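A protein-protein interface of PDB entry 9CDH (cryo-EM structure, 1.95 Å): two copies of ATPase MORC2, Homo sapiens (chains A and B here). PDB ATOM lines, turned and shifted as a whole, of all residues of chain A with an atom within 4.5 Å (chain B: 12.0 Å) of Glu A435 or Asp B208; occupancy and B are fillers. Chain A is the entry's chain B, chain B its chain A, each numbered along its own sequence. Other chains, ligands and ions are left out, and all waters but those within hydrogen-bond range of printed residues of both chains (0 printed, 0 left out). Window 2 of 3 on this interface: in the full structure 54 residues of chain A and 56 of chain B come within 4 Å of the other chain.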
ATOM      1  N   ARG A 283      30.627 -14.158 -15.500  1.00  0.00           N
ATOM      2  CA  ARG A 283      30.108 -14.643 -16.773  1.00  0.00           C
ATOM      3  C   ARG A 283      30.163 -13.556 -17.837  1.00  0.00           C
ATOM      4  O   ARG A 283      30.535 -13.823 -18.986  1.00  0.00           O
ATOM      5  CB  ARG A 283      28.674 -15.144 -16.617  1.00  0.00           C
ATOM      6  CG  ARG A 283      27.964 -15.304 -17.953  1.00  0.00           C
ATOM      7  CD  ARG A 283      26.732 -16.176 -17.850  1.00  0.00           C
ATOM      8  NE  ARG A 283      27.070 -17.594 -17.883  1.00  0.00           N
ATOM      9  CZ  ARG A 283      26.299 -18.542 -18.400  1.00  0.00           C
ATOM     10  NH1 ARG A 283      25.126 -18.262 -18.945  1.00  0.00           N
ATOM     11  NH2 ARG A 283      26.711 -19.805 -18.360  1.00  0.00           N
ATOM     12  N   ARG A 287      32.337 -14.128 -21.255  1.00  0.00           N
ATOM     13  CA  ARG A 287      31.740 -14.058 -22.581  1.00  0.00           C
ATOM     14  C   ARG A 287      32.096 -12.774 -23.318  1.00  0.00           C
ATOM     15  O   ARG A 287      31.901 -12.712 -24.538  1.00  0.00           O
ATOM     16  CB  ARG A 287      30.223 -14.225 -22.484  1.00  0.00           C
ATOM     17  CG  ARG A 287      29.813 -15.400 -21.603  1.00  0.00           C
ATOM     18  CD  ARG A 287      28.611 -16.150 -22.155  1.00  0.00           C
ATOM     19  NE  ARG A 287      28.562 -17.518 -21.651  1.00  0.00           N
ATOM     20  CZ  ARG A 287      27.460 -18.250 -21.562  1.00  0.00           C
ATOM     21  NH1 ARG A 287      26.279 -17.774 -21.927  1.00  0.00           N
ATOM     22  NH2 ARG A 287      27.543 -19.493 -21.097  1.00  0.00           N
ATOM     23  N   LEU A 421      22.842 -13.809 -19.583  1.00  0.00           N
ATOM     24  CA  LEU A 421      21.794 -14.806 -19.444  1.00  0.00           C
ATOM     25  C   LEU A 421      21.052 -14.924 -20.761  1.00  0.00           C
ATOM     26  O   LEU A 421      20.940 -13.951 -21.509  1.00  0.00           O
ATOM     27  CB  LEU A 421      20.811 -14.439 -18.326  1.00  0.00           C
ATOM     28  CG  LEU A 421      21.281 -14.627 -16.885  1.00  0.00           C
ATOM     29  CD1 LEU A 421      20.181 -14.221 -15.923  1.00  0.00           C
ATOM     30  CD2 LEU A 421      21.699 -16.064 -16.636  1.00  0.00           C
ATOM     31  N   ASP A 432      19.791 -20.742 -18.379  1.00  0.00           N
ATOM     32  CA  ASP A 432      20.834 -21.176 -17.453  1.00  0.00           C
ATOM     33  C   ASP A 432      20.321 -20.941 -16.038  1.00  0.00           C
ATOM     34  O   ASP A 432      20.434 -19.847 -15.486  1.00  0.00           O
ATOM     35  CB  ASP A 432      22.139 -20.435 -17.717  1.00  0.00           C
ATOM     36  CG  ASP A 432      23.316 -21.053 -16.994  1.00  0.00           C
ATOM     37  OD1 ASP A 432      23.132 -21.538 -15.858  1.00  0.00           O
ATOM     38  OD2 ASP A 432      24.425 -21.060 -17.566  1.00  0.00           O
ATOM     39  N   ALA A 433      19.751 -21.993 -15.447  1.00  0.00           N
ATOM     40  CA  ALA A 433      19.168 -21.871 -14.116  1.00  0.00           C
ATOM     41  C   ALA A 433      20.217 -21.525 -13.069  1.00  0.00           C
ATOM     42  O   ALA A 433      19.950 -20.723 -12.170  1.00  0.00           O
ATOM     43  CB  ALA A 433      18.452 -23.167 -13.739  1.00  0.00           C
ATOM     44  N   LYS A 434      21.407 -22.120 -13.159  1.00  0.00           N
ATOM     45  CA  LYS A 434      22.445 -21.847 -12.168  1.00  0.00           C
ATOM     46  C   LYS A 434      22.852 -20.380 -12.190  1.00  0.00           C
ATOM     47  O   LYS A 434      22.945 -19.732 -11.141  1.00  0.00           O
ATOM     48  CB  LYS A 434      23.656 -22.743 -12.425  1.00  0.00           C
ATOM     49  CG  LYS A 434      24.842 -22.457 -11.520  1.00  0.00           C
ATOM     50  CD  LYS A 434      25.950 -23.476 -11.719  1.00  0.00           C
ATOM     51  CE  LYS A 434      27.080 -23.269 -10.725  1.00  0.00           C
ATOM     52  NZ  LYS A 434      28.064 -22.261 -11.203  1.00  0.00           N
ATOM     53  N   GLU A 435      23.093 -19.835 -13.381  1.00  0.00           N
ATOM     54  CA  GLU A 435      23.524 -18.446 -13.464  1.00  0.00           C
ATOM     55  C   GLU A 435      22.382 -17.489 -13.164  1.00  0.00           C
ATOM     56  O   GLU A 435      22.615 -16.402 -12.629  1.00  0.00           O
ATOM     57  CB  GLU A 435      24.121 -18.164 -14.839  1.00  0.00           C
ATOM     58  CG  GLU A 435      25.533 -18.698 -14.999  1.00  0.00           C
ATOM     59  CD  GLU A 435      26.501 -18.119 -13.984  1.00  0.00           C
ATOM     60  OE1 GLU A 435      26.435 -16.898 -13.726  1.00  0.00           O
ATOM     61  OE2 GLU A 435      27.324 -18.884 -13.442  1.00  0.00           O
ATOM     62  N   TYR A 436      21.144 -17.873 -13.478  1.00  0.00           N
ATOM     63  CA  TYR A 436      20.012 -17.065 -13.046  1.00  0.00           C
ATOM     64  C   TYR A 436      19.918 -17.028 -11.527  1.00  0.00           C
ATOM     65  O   TYR A 436      19.623 -15.981 -10.943  1.00  0.00           O
ATOM     66  CB  TYR A 436      18.711 -17.593 -13.644  1.00  0.00           C
ATOM     67  CG  TYR A 436      17.499 -16.860 -13.124  1.00  0.00           C
ATOM     68  CD1 TYR A 436      17.398 -15.482 -13.240  1.00  0.00           C
ATOM     69  CD2 TYR A 436      16.458 -17.542 -12.513  1.00  0.00           C
ATOM     70  CE1 TYR A 436      16.297 -14.804 -12.765  1.00  0.00           C
ATOM     71  CE2 TYR A 436      15.352 -16.872 -12.035  1.00  0.00           C
ATOM     72  CZ  TYR A 436      15.276 -15.503 -12.167  1.00  0.00           C
ATOM     73  OH  TYR A 436      14.177 -14.832 -11.692  1.00  0.00           O
ATOM     74  N   ARG A 437      20.149 -18.166 -10.869  1.00  0.00           N
ATOM     75  CA  ARG A 437      20.157 -18.185  -9.410  1.00  0.00           C
ATOM     76  C   ARG A 437      21.281 -17.321  -8.862  1.00  0.00           C
ATOM     77  O   ARG A 437      21.106 -16.625  -7.857  1.00  0.00           O
ATOM     78  CB  ARG A 437      20.291 -19.620  -8.902  1.00  0.00           C
ATOM     79  CG  ARG A 437      18.991 -20.400  -8.893  1.00  0.00           C
ATOM     80  CD  ARG A 437      19.141 -21.705  -8.131  1.00  0.00           C
ATOM     81  NE  ARG A 437      19.971 -22.662  -8.851  1.00  0.00           N
ATOM     82  CZ  ARG A 437      19.542 -23.424  -9.849  1.00  0.00           C
ATOM     83  NH1 ARG A 437      18.288 -23.375 -10.267  1.00  0.00           N
ATOM     84  NH2 ARG A 437      20.394 -24.255 -10.441  1.00  0.00           N
ATOM     85  N   HIS A 438      22.449 -17.363  -9.501  1.00  0.00           N
ATOM     86  CA  HIS A 438      23.551 -16.500  -9.088  1.00  0.00           C
ATOM     87  C   HIS A 438      23.165 -15.029  -9.210  1.00  0.00           C
ATOM     88  O   HIS A 438      23.434 -14.223  -8.310  1.00  0.00           O
ATOM     89  CB  HIS A 438      24.791 -16.803  -9.928  1.00  0.00           C
ATOM     90  CG  HIS A 438      26.039 -16.160  -9.413  1.00  0.00           C
ATOM     91  ND1 HIS A 438      26.745 -16.656  -8.339  1.00  0.00           N
ATOM     92  CD2 HIS A 438      26.708 -15.057  -9.825  1.00  0.00           C
ATOM     93  CE1 HIS A 438      27.796 -15.888  -8.112  1.00  0.00           C
ATOM     94  NE2 HIS A 438      27.796 -14.910  -9.000  1.00  0.00           N
ATOM     95  N   LEU A 439      22.533 -14.663 -10.326  1.00  0.00           N
ATOM     96  CA  LEU A 439      22.103 -13.285 -10.517  1.00  0.00           C
ATOM     97  C   LEU A 439      21.059 -12.888  -9.482  1.00  0.00           C
ATOM     98  O   LEU A 439      21.078 -11.766  -8.971  1.00  0.00           O
ATOM     99  CB  LEU A 439      21.554 -13.096 -11.931  1.00  0.00           C
ATOM    100  CG  LEU A 439      20.922 -11.733 -12.217  1.00  0.00           C
ATOM    101  CD1 LEU A 439      21.537 -11.115 -13.457  1.00  0.00           C
ATOM    102  CD2 LEU A 439      19.417 -11.859 -12.365  1.00  0.00           C
ATOM    103  N   HIS B  26      14.391 -26.575 -21.322  1.00  0.00           N
ATOM    104  CA  HIS B  26      14.776 -27.271 -20.095  1.00  0.00           C
ATOM    105  C   HIS B  26      15.723 -26.388 -19.291  1.00  0.00           C
ATOM    106  O   HIS B  26      16.942 -26.545 -19.345  1.00  0.00           O
ATOM    107  CB  HIS B  26      15.424 -28.611 -20.419  1.00  0.00           C
ATOM    108  CG  HIS B  26      14.511 -29.579 -21.100  1.00  0.00           C
ATOM    109  ND1 HIS B  26      13.443 -30.170 -20.462  1.00  0.00           N
ATOM    110  CD2 HIS B  26      14.515 -30.070 -22.361  1.00  0.00           C
ATOM    111  CE1 HIS B  26      12.824 -30.978 -21.302  1.00  0.00           C
ATOM    112  NE2 HIS B  26      13.456 -30.937 -22.460  1.00  0.00           N
ATOM    113  N   GLU B  27      15.157 -25.454 -18.527  1.00  0.00           N
ATOM    114  CA  GLU B  27      15.960 -24.770 -17.520  1.00  0.00           C
ATOM    115  C   GLU B  27      16.290 -25.712 -16.371  1.00  0.00           C
ATOM    116  O   GLU B  27      17.287 -25.512 -15.670  1.00  0.00           O
ATOM    117  CB  GLU B  27      15.229 -23.526 -17.012  1.00  0.00           C
ATOM    118  CG  GLU B  27      13.933 -23.806 -16.263  1.00  0.00           C
ATOM    119  CD  GLU B  27      14.144 -24.072 -14.782  1.00  0.00           C
ATOM    120  OE1 GLU B  27      15.267 -23.849 -14.283  1.00  0.00           O
ATOM    121  OE2 GLU B  27      13.182 -24.505 -14.114  1.00  0.00           O
ATOM    122  N   PHE B  28      15.464 -26.735 -16.172  1.00  0.00           N
ATOM    123  CA  PHE B  28      15.721 -27.800 -15.212  1.00  0.00           C
ATOM    124  C   PHE B  28      16.396 -28.945 -15.961  1.00  0.00           C
ATOM    125  O   PHE B  28      15.751 -29.642 -16.750  1.00  0.00           O
ATOM    126  CB  PHE B  28      14.408 -28.237 -14.567  1.00  0.00           C
ATOM    127  CG  PHE B  28      14.566 -29.206 -13.434  1.00  0.00           C
ATOM    128  CD1 PHE B  28      15.463 -28.965 -12.410  1.00  0.00           C
ATOM    129  CD2 PHE B  28      13.785 -30.347 -13.376  1.00  0.00           C
ATOM    130  CE1 PHE B  28      15.594 -29.853 -11.365  1.00  0.00           C
ATOM    131  CE2 PHE B  28      13.912 -31.235 -12.332  1.00  0.00           C
ATOM    132  CZ  PHE B  28      14.814 -30.985 -11.322  1.00  0.00           C
ATOM    133  N   LEU B  29      17.698 -29.123 -15.731  1.00  0.00           N
ATOM    134  CA  LEU B  29      18.460 -30.120 -16.480  1.00  0.00           C
ATOM    135  C   LEU B  29      18.001 -31.539 -16.162  1.00  0.00           C
ATOM    136  O   LEU B  29      18.002 -32.413 -17.042  1.00  0.00           O
ATOM    137  CB  LEU B  29      19.948 -29.952 -16.177  1.00  0.00           C
ATOM    138  CG  LEU B  29      20.935 -30.873 -16.893  1.00  0.00           C
ATOM    139  CD1 LEU B  29      20.759 -30.803 -18.398  1.00  0.00           C
ATOM    140  CD2 LEU B  29      22.352 -30.501 -16.505  1.00  0.00           C
ATOM    141  N   ARG B  59      34.054 -33.197 -24.519  1.00  0.00           N
ATOM    142  CA  ARG B  59      33.726 -32.101 -23.621  1.00  0.00           C
ATOM    143  C   ARG B  59      32.895 -32.615 -22.453  1.00  0.00           C
ATOM    144  O   ARG B  59      31.922 -33.349 -22.640  1.00  0.00           O
ATOM    145  CB  ARG B  59      32.971 -31.011 -24.378  1.00  0.00           C
ATOM    146  CG  ARG B  59      32.764 -29.744 -23.579  1.00  0.00           C
ATOM    147  CD  ARG B  59      31.995 -28.717 -24.377  1.00  0.00           C
ATOM    148  NE  ARG B  59      30.564 -28.991 -24.369  1.00  0.00           N
ATOM    149  CZ  ARG B  59      29.699 -28.482 -25.233  1.00  0.00           C
ATOM    150  NH1 ARG B  59      30.082 -27.648 -26.186  1.00  0.00           N
ATOM    151  NH2 ARG B  59      28.417 -28.821 -25.144  1.00  0.00           N
ATOM    152  N   GLY B  60      33.290 -32.230 -21.244  1.00  0.00           N
ATOM    153  CA  GLY B  60      32.698 -32.735 -20.029  1.00  0.00           C
ATOM    154  C   GLY B  60      33.439 -33.908 -19.422  1.00  0.00           C
ATOM    155  O   GLY B  60      33.242 -34.201 -18.238  1.00  0.00           O
ATOM    156  N   ARG B 110      19.638 -30.323 -24.550  1.00  0.00           N
ATOM    157  CA  ARG B 110      19.931 -29.564 -23.341  1.00  0.00           C
ATOM    158  C   ARG B 110      21.113 -30.157 -22.585  1.00  0.00           C
ATOM    159  O   ARG B 110      21.950 -29.413 -22.064  1.00  0.00           O
ATOM    160  CB  ARG B 110      18.700 -29.514 -22.440  1.00  0.00           C
ATOM    161  CG  ARG B 110      18.953 -28.927 -21.060  1.00  0.00           C
ATOM    162  CD  ARG B 110      19.257 -27.444 -21.130  1.00  0.00           C
ATOM    163  NE  ARG B 110      19.612 -26.909 -19.822  1.00  0.00           N
ATOM    164  CZ  ARG B 110      20.817 -26.993 -19.276  1.00  0.00           C
ATOM    165  NH1 ARG B 110      21.824 -27.573 -19.907  1.00  0.00           N
ATOM    166  NH2 ARG B 110      21.015 -26.484 -18.064  1.00  0.00           N
ATOM    167  N   LEU B 204      29.155 -32.882 -23.346  1.00  0.00           N
ATOM    168  CA  LEU B 204      28.185 -32.327 -22.420  1.00  0.00           C
ATOM    169  C   LEU B 204      28.420 -30.835 -22.216  1.00  0.00           C
ATOM    170  O   LEU B 204      29.535 -30.324 -22.345  1.00  0.00           O
ATOM    171  CB  LEU B 204      28.254 -33.052 -21.077  1.00  0.00           C
ATOM    172  CG  LEU B 204      28.250 -34.580 -21.151  1.00  0.00           C
ATOM    173  CD1 LEU B 204      28.422 -35.168 -19.769  1.00  0.00           C
ATOM    174  CD2 LEU B 204      26.973 -35.089 -21.795  1.00  0.00           C
ATOM    175  N   LYS B 205      27.339 -30.135 -21.894  1.00  0.00           N
ATOM    176  CA  LYS B 205      27.422 -28.706 -21.649  1.00  0.00           C
ATOM    177  C   LYS B 205      28.328 -28.435 -20.457  1.00  0.00           C
ATOM    178  O   LYS B 205      28.254 -29.117 -19.431  1.00  0.00           O
ATOM    179  CB  LYS B 205      26.034 -28.126 -21.385  1.00  0.00           C
ATOM    180  CG  LYS B 205      24.988 -28.478 -22.430  1.00  0.00           C
ATOM    181  CD  LYS B 205      25.395 -28.037 -23.818  1.00  0.00           C
ATOM    182  CE  LYS B 205      24.253 -28.200 -24.802  1.00  0.00           C
ATOM    183  NZ  LYS B 205      23.123 -27.283 -24.497  1.00  0.00           N
ATOM    184  N   LEU B 206      29.187 -27.434 -20.595  1.00  0.00           N
ATOM    185  CA  LEU B 206      30.073 -27.021 -19.522  1.00  0.00           C
ATOM    186  C   LEU B 206      29.522 -25.778 -18.841  1.00  0.00           C
ATOM    187  O   LEU B 206      28.865 -24.942 -19.464  1.00  0.00           O
ATOM    188  CB  LEU B 206      31.481 -26.734 -20.044  1.00  0.00           C
ATOM    189  CG  LEU B 206      32.184 -27.861 -20.796  1.00  0.00           C
ATOM    190  CD1 LEU B 206      33.557 -27.396 -21.251  1.00  0.00           C
ATOM    191  CD2 LEU B 206      32.282 -29.110 -19.936  1.00  0.00           C
ATOM    192  N   MET B 207      29.786 -25.672 -17.545  1.00  0.00           N
ATOM    193  CA  MET B 207      29.494 -24.444 -16.833  1.00  0.00           C
ATOM    194  C   MET B 207      30.531 -23.382 -17.191  1.00  0.00           C
ATOM    195  O   MET B 207      31.392 -23.575 -18.054  1.00  0.00           O
ATOM    196  CB  MET B 207      29.474 -24.693 -15.327  1.00  0.00           C
ATOM    197  CG  MET B 207      28.444 -25.716 -14.889  1.00  0.00           C
ATOM    198  SD  MET B 207      28.334 -25.864 -13.100  1.00  0.00           S
ATOM    199  CE  MET B 207      29.971 -26.471 -12.707  1.00  0.00           C
ATOM    200  N   ASP B 208      30.437 -22.238 -16.512  1.00  0.00           N
ATOM    201  CA  ASP B 208      31.370 -21.148 -16.774  1.00  0.00           C
ATOM    202  C   ASP B 208      32.801 -21.559 -16.458  1.00  0.00           C
ATOM    203  O   ASP B 208      33.733 -21.218 -17.195  1.00  0.00           O
ATOM    204  CB  ASP B 208      30.974 -19.924 -15.952  1.00  0.00           C
ATOM    205  CG  ASP B 208      29.997 -19.028 -16.678  1.00  0.00           C
ATOM    206  OD1 ASP B 208      29.444 -18.119 -16.030  1.00  0.00           O
ATOM    207  OD2 ASP B 208      29.780 -19.227 -17.892  1.00  0.00           O
ATOM    208  N   ASN B 209      32.994 -22.299 -15.368  1.00  0.00           N
ATOM    209  CA  ASN B 209      34.321 -22.734 -14.953  1.00  0.00           C
ATOM    210  C   ASN B 209      34.897 -23.833 -15.835  1.00  0.00           C
ATOM    211  O   ASN B 209      35.983 -24.335 -15.527  1.00  0.00           O
ATOM    212  CB  ASN B 209      34.273 -23.214 -13.503  1.00  0.00           C
ATOM    213  CG  ASN B 209      33.376 -24.420 -13.319  1.00  0.00           C
ATOM    214  OD1 ASN B 209      32.793 -24.928 -14.276  1.00  0.00           O
ATOM    215  ND2 ASN B 209      33.256 -24.882 -12.081  1.00  0.00           N
ATOM    216  N   GLY B 210      34.212 -24.222 -16.908  1.00  0.00           N
ATOM    217  CA  GLY B 210      34.682 -25.280 -17.772  1.00  0.00           C
ATOM    218  C   GLY B 210      34.343 -26.678 -17.310  1.00  0.00           C
ATOM    219  O   GLY B 210      34.693 -27.641 -18.003  1.00  0.00           O
ATOM    220  N   GLU B 211      33.684 -26.825 -16.173  1.00  0.00           N
ATOM    221  CA  GLU B 211      33.279 -28.136 -15.697  1.00  0.00           C
ATOM    222  C   GLU B 211      31.904 -28.495 -16.248  1.00  0.00           C
ATOM    223  O   GLU B 211      31.092 -27.609 -16.531  1.00  0.00           O
ATOM    224  CB  GLU B 211      33.235 -28.155 -14.172  1.00  0.00           C
ATOM    225  CG  GLU B 211      34.601 -28.157 -13.511  1.00  0.00           C
ATOM    226  CD  GLU B 211      35.329 -29.473 -13.679  1.00  0.00           C
ATOM    227  OE1 GLU B 211      35.944 -29.681 -14.744  1.00  0.00           O
ATOM    228  OE2 GLU B 211      35.284 -30.302 -12.745  1.00  0.00           O
ATOM    229  N   PRO B 212      31.605 -29.779 -16.425  1.00  0.00           N
ATOM    230  CA  PRO B 212      30.258 -30.159 -16.858  1.00  0.00           C
ATOM    231  C   PRO B 212      29.215 -29.805 -15.809  1.00  0.00           C
ATOM    232  O   PRO B 212      29.479 -29.823 -14.605  1.00  0.00           O
ATOM    233  CB  PRO B 212      30.358 -31.677 -17.057  1.00  0.00           C
ATOM    234  CG  PRO B 212      31.528 -32.100 -16.252  1.00  0.00           C
ATOM    235  CD  PRO B 212      32.480 -30.950 -16.242  1.00  0.00           C
ATOM    236  N   GLU B 213      28.013 -29.472 -16.284  1.00  0.00           N
ATOM    237  CA  GLU B 213      26.926 -29.162 -15.363  1.00  0.00           C
ATOM    238  C   GLU B 213      26.563 -30.364 -14.507  1.00  0.00           C
ATOM    239  O   GLU B 213      26.134 -30.205 -13.360  1.00  0.00           O
ATOM    240  CB  GLU B 213      25.686 -28.689 -16.122  1.00  0.00           C
ATOM    241  CG  GLU B 213      25.943 -27.718 -17.250  1.00  0.00           C
ATOM    242  CD  GLU B 213      24.654 -27.234 -17.879  1.00  0.00           C
ATOM    243  OE1 GLU B 213      24.096 -26.227 -17.396  1.00  0.00           O
ATOM    244  OE2 GLU B 213      24.188 -27.870 -18.846  1.00  0.00           O
ATOM    245  N   LEU B 214      26.716 -31.568 -15.047  1.00  0.00           N
ATOM    246  CA  LEU B 214      26.387 -32.796 -14.342  1.00  0.00           C
ATOM    247  C   LEU B 214      27.623 -33.277 -13.597  1.00  0.00           C
ATOM    248  O   LEU B 214      28.646 -33.584 -14.216  1.00  0.00           O
ATOM    249  CB  LEU B 214      25.888 -33.862 -15.315  1.00  0.00           C
ATOM    250  CG  LEU B 214      24.596 -33.498 -16.048  1.00  0.00           C
ATOM    251  CD1 LEU B 214      24.280 -34.534 -17.107  1.00  0.00           C
ATOM    252  CD2 LEU B 214      23.438 -33.351 -15.070  1.00  0.00           C
ATOM    253  N   MET B 225      23.735 -32.012  -9.785  1.00  0.00           N
ATOM    254  CA  MET B 225      23.941 -30.697 -10.370  1.00  0.00           C
ATOM    255  C   MET B 225      25.238 -30.120  -9.825  1.00  0.00           C
ATOM    256  O   MET B 225      25.443 -30.075  -8.609  1.00  0.00           O
ATOM    257  CB  MET B 225      22.770 -29.771 -10.045  1.00  0.00           C
ATOM    258  CG  MET B 225      21.453 -30.151 -10.706  1.00  0.00           C
ATOM    259  SD  MET B 225      21.564 -30.358 -12.493  1.00  0.00           S
ATOM    260  CE  MET B 225      22.017 -28.703 -12.995  1.00  0.00           C
ATOM    261  N   ALA B 226      26.115 -29.682 -10.723  1.00  0.00           N
ATOM    262  CA  ALA B 226      27.389 -29.115 -10.304  1.00  0.00           C
ATOM    263  C   ALA B 226      27.164 -27.720  -9.739  1.00  0.00           C
ATOM    264  O   ALA B 226      27.296 -26.722 -10.454  1.00  0.00           O
ATOM    265  CB  ALA B 226      28.371 -29.079 -11.474  1.00  0.00           C
ATOM    266  N   GLU B 227      26.819 -27.643  -8.456  1.00  0.00           N
ATOM    267  CA  GLU B 227      26.464 -26.374  -7.835  1.00  0.00           C
ATOM    268  C   GLU B 227      26.264 -26.535  -6.333  1.00  0.00           C
ATOM    269  O   GLU B 227      25.935 -27.626  -5.856  1.00  0.00           O
ATOM    270  CB  GLU B 227      25.210 -25.801  -8.503  1.00  0.00           C
ATOM    271  CG  GLU B 227      24.043 -26.782  -8.638  1.00  0.00           C
ATOM    272  CD  GLU B 227      23.449 -27.207  -7.311  1.00  0.00           C
ATOM    273  OE1 GLU B 227      22.914 -26.338  -6.595  1.00  0.00           O
ATOM    274  OE2 GLU B 227      23.519 -28.409  -6.982  1.00  0.00           O
ATOM    275  N   THR B 228      26.460 -25.453  -5.583  1.00  0.00           N
ATOM    276  CA  THR B 228      26.337 -25.510  -4.134  1.00  0.00           C
ATOM    277  C   THR B 228      24.933 -25.954  -3.734  1.00  0.00           C
ATOM    278  O   THR B 228      23.961 -25.783  -4.474  1.00  0.00           O
ATOM    279  CB  THR B 228      26.646 -24.149  -3.510  1.00  0.00           C
ATOM    280  OG1 THR B 228      26.345 -24.183  -2.109  1.00  0.00           O
ATOM    281  CG2 THR B 228      25.823 -23.047  -4.171  1.00  0.00           C
ATOM    282  N   PRO B 230      22.345 -25.025  -1.257  1.00  0.00           N
ATOM    283  CA  PRO B 230      21.736 -24.193  -0.212  1.00  0.00           C
ATOM    284  C   PRO B 230      20.920 -25.007   0.776  1.00  0.00           C
ATOM    285  O   PRO B 230      20.515 -26.135   0.481  1.00  0.00           O
ATOM    286  CB  PRO B 230      20.851 -23.226  -1.006  1.00  0.00           C
ATOM    287  CG  PRO B 230      21.507 -23.114  -2.332  1.00  0.00           C
ATOM    288  CD  PRO B 230      22.244 -24.403  -2.589  1.00  0.00           C
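Of the 23 printed residues of chain B, 5 touch a printed residue of chain A.
Along chain B the printed residues that touch a printed residue of chain A span positions 27 to 227.
Hydrophobic or aromatic side chains of chain A that line the printed part of chain B: Ala A433.
Among the printed residues, Asp or Glu carboxylates within 4 Å of a Lys or Arg side-chain nitrogen of the other chain: Arg A283 with Asp B208 (3.1 Å) and Arg A287 with Asp B208 (3.9 Å).
No position is printed for both chains.
Of the 7 pairs that touch across the chains among the printed residues, none has its exchanged pair printed and touching as well.
Printed residues of chain B within 4 Å of Arg A287: Asp B208 (3.9 Å).
Ala A433 touches just one residue of chain B: Glu B27 (3.3 Å).
Glu A435 touches just one residue of chain B: Asp B208.
His A438 touches none of the printed residues of chain B.
No residue of chain B comes within 4 Å of Leu A439.
Of the printed residues of chain A, Glu B27 touches Ala A433 (3.3 Å).
Of the printed residues of chain A, Met B207 touches Lys A434.
Printed residues of chain A within 4 Å of Asp B208: Arg A283, Arg A287 and Glu A435.
Of the printed residues of chain A, Ala B226 touches Lys A434 (3.5 Å).
Printed residues of chain A within 4 Å of Glu B227: Lys A434.
The nearest residue of chain B that does not touch Glu A435 is Met B207 (6.5 Å).
The nearest printed residue of chain A that does not touch Asp B208 is Asp A432 (5.7 Å).
NE of Arg A283 is in salt-bridge range of OD1 of Asp B208, 3.1 Å away.
The guanidinium group (NH2) of Arg A287 is in salt-bridge range of the side-chain carboxylate (OD2) of Asp B208 (3.9 Å).
OE2 of Glu A435 lies close to OD1 of Asp B208 (3.4 Å).
The backbone carbonyl oxygen (O) of Glu B213 is in hydrogen-bond range of the backbone NH (N) of Ala B226, at 2.7 Å.
OD2 of Asp A432 is in salt-bridge range of NH2 of Arg A283, 2.7 Å away.
The backbone NH of Lys A434 sits at hydrogen-bond distance from the side-chain carboxylate of Asp A432 (3.3 Å).
The backbone NH of Glu A435 lies within hydrogen-bond range of the side-chain carboxylate of Asp A432 (3.0 Å).
Among the printed residues, merely in contact across the chains: Ala A433 with Glu B27 (3.3 Å), Lys A434 with Ala B226 (3.5 Å), Lys A434 with Met B207 (3.6 Å) and Lys A434 with Glu B227 (3.9 Å).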
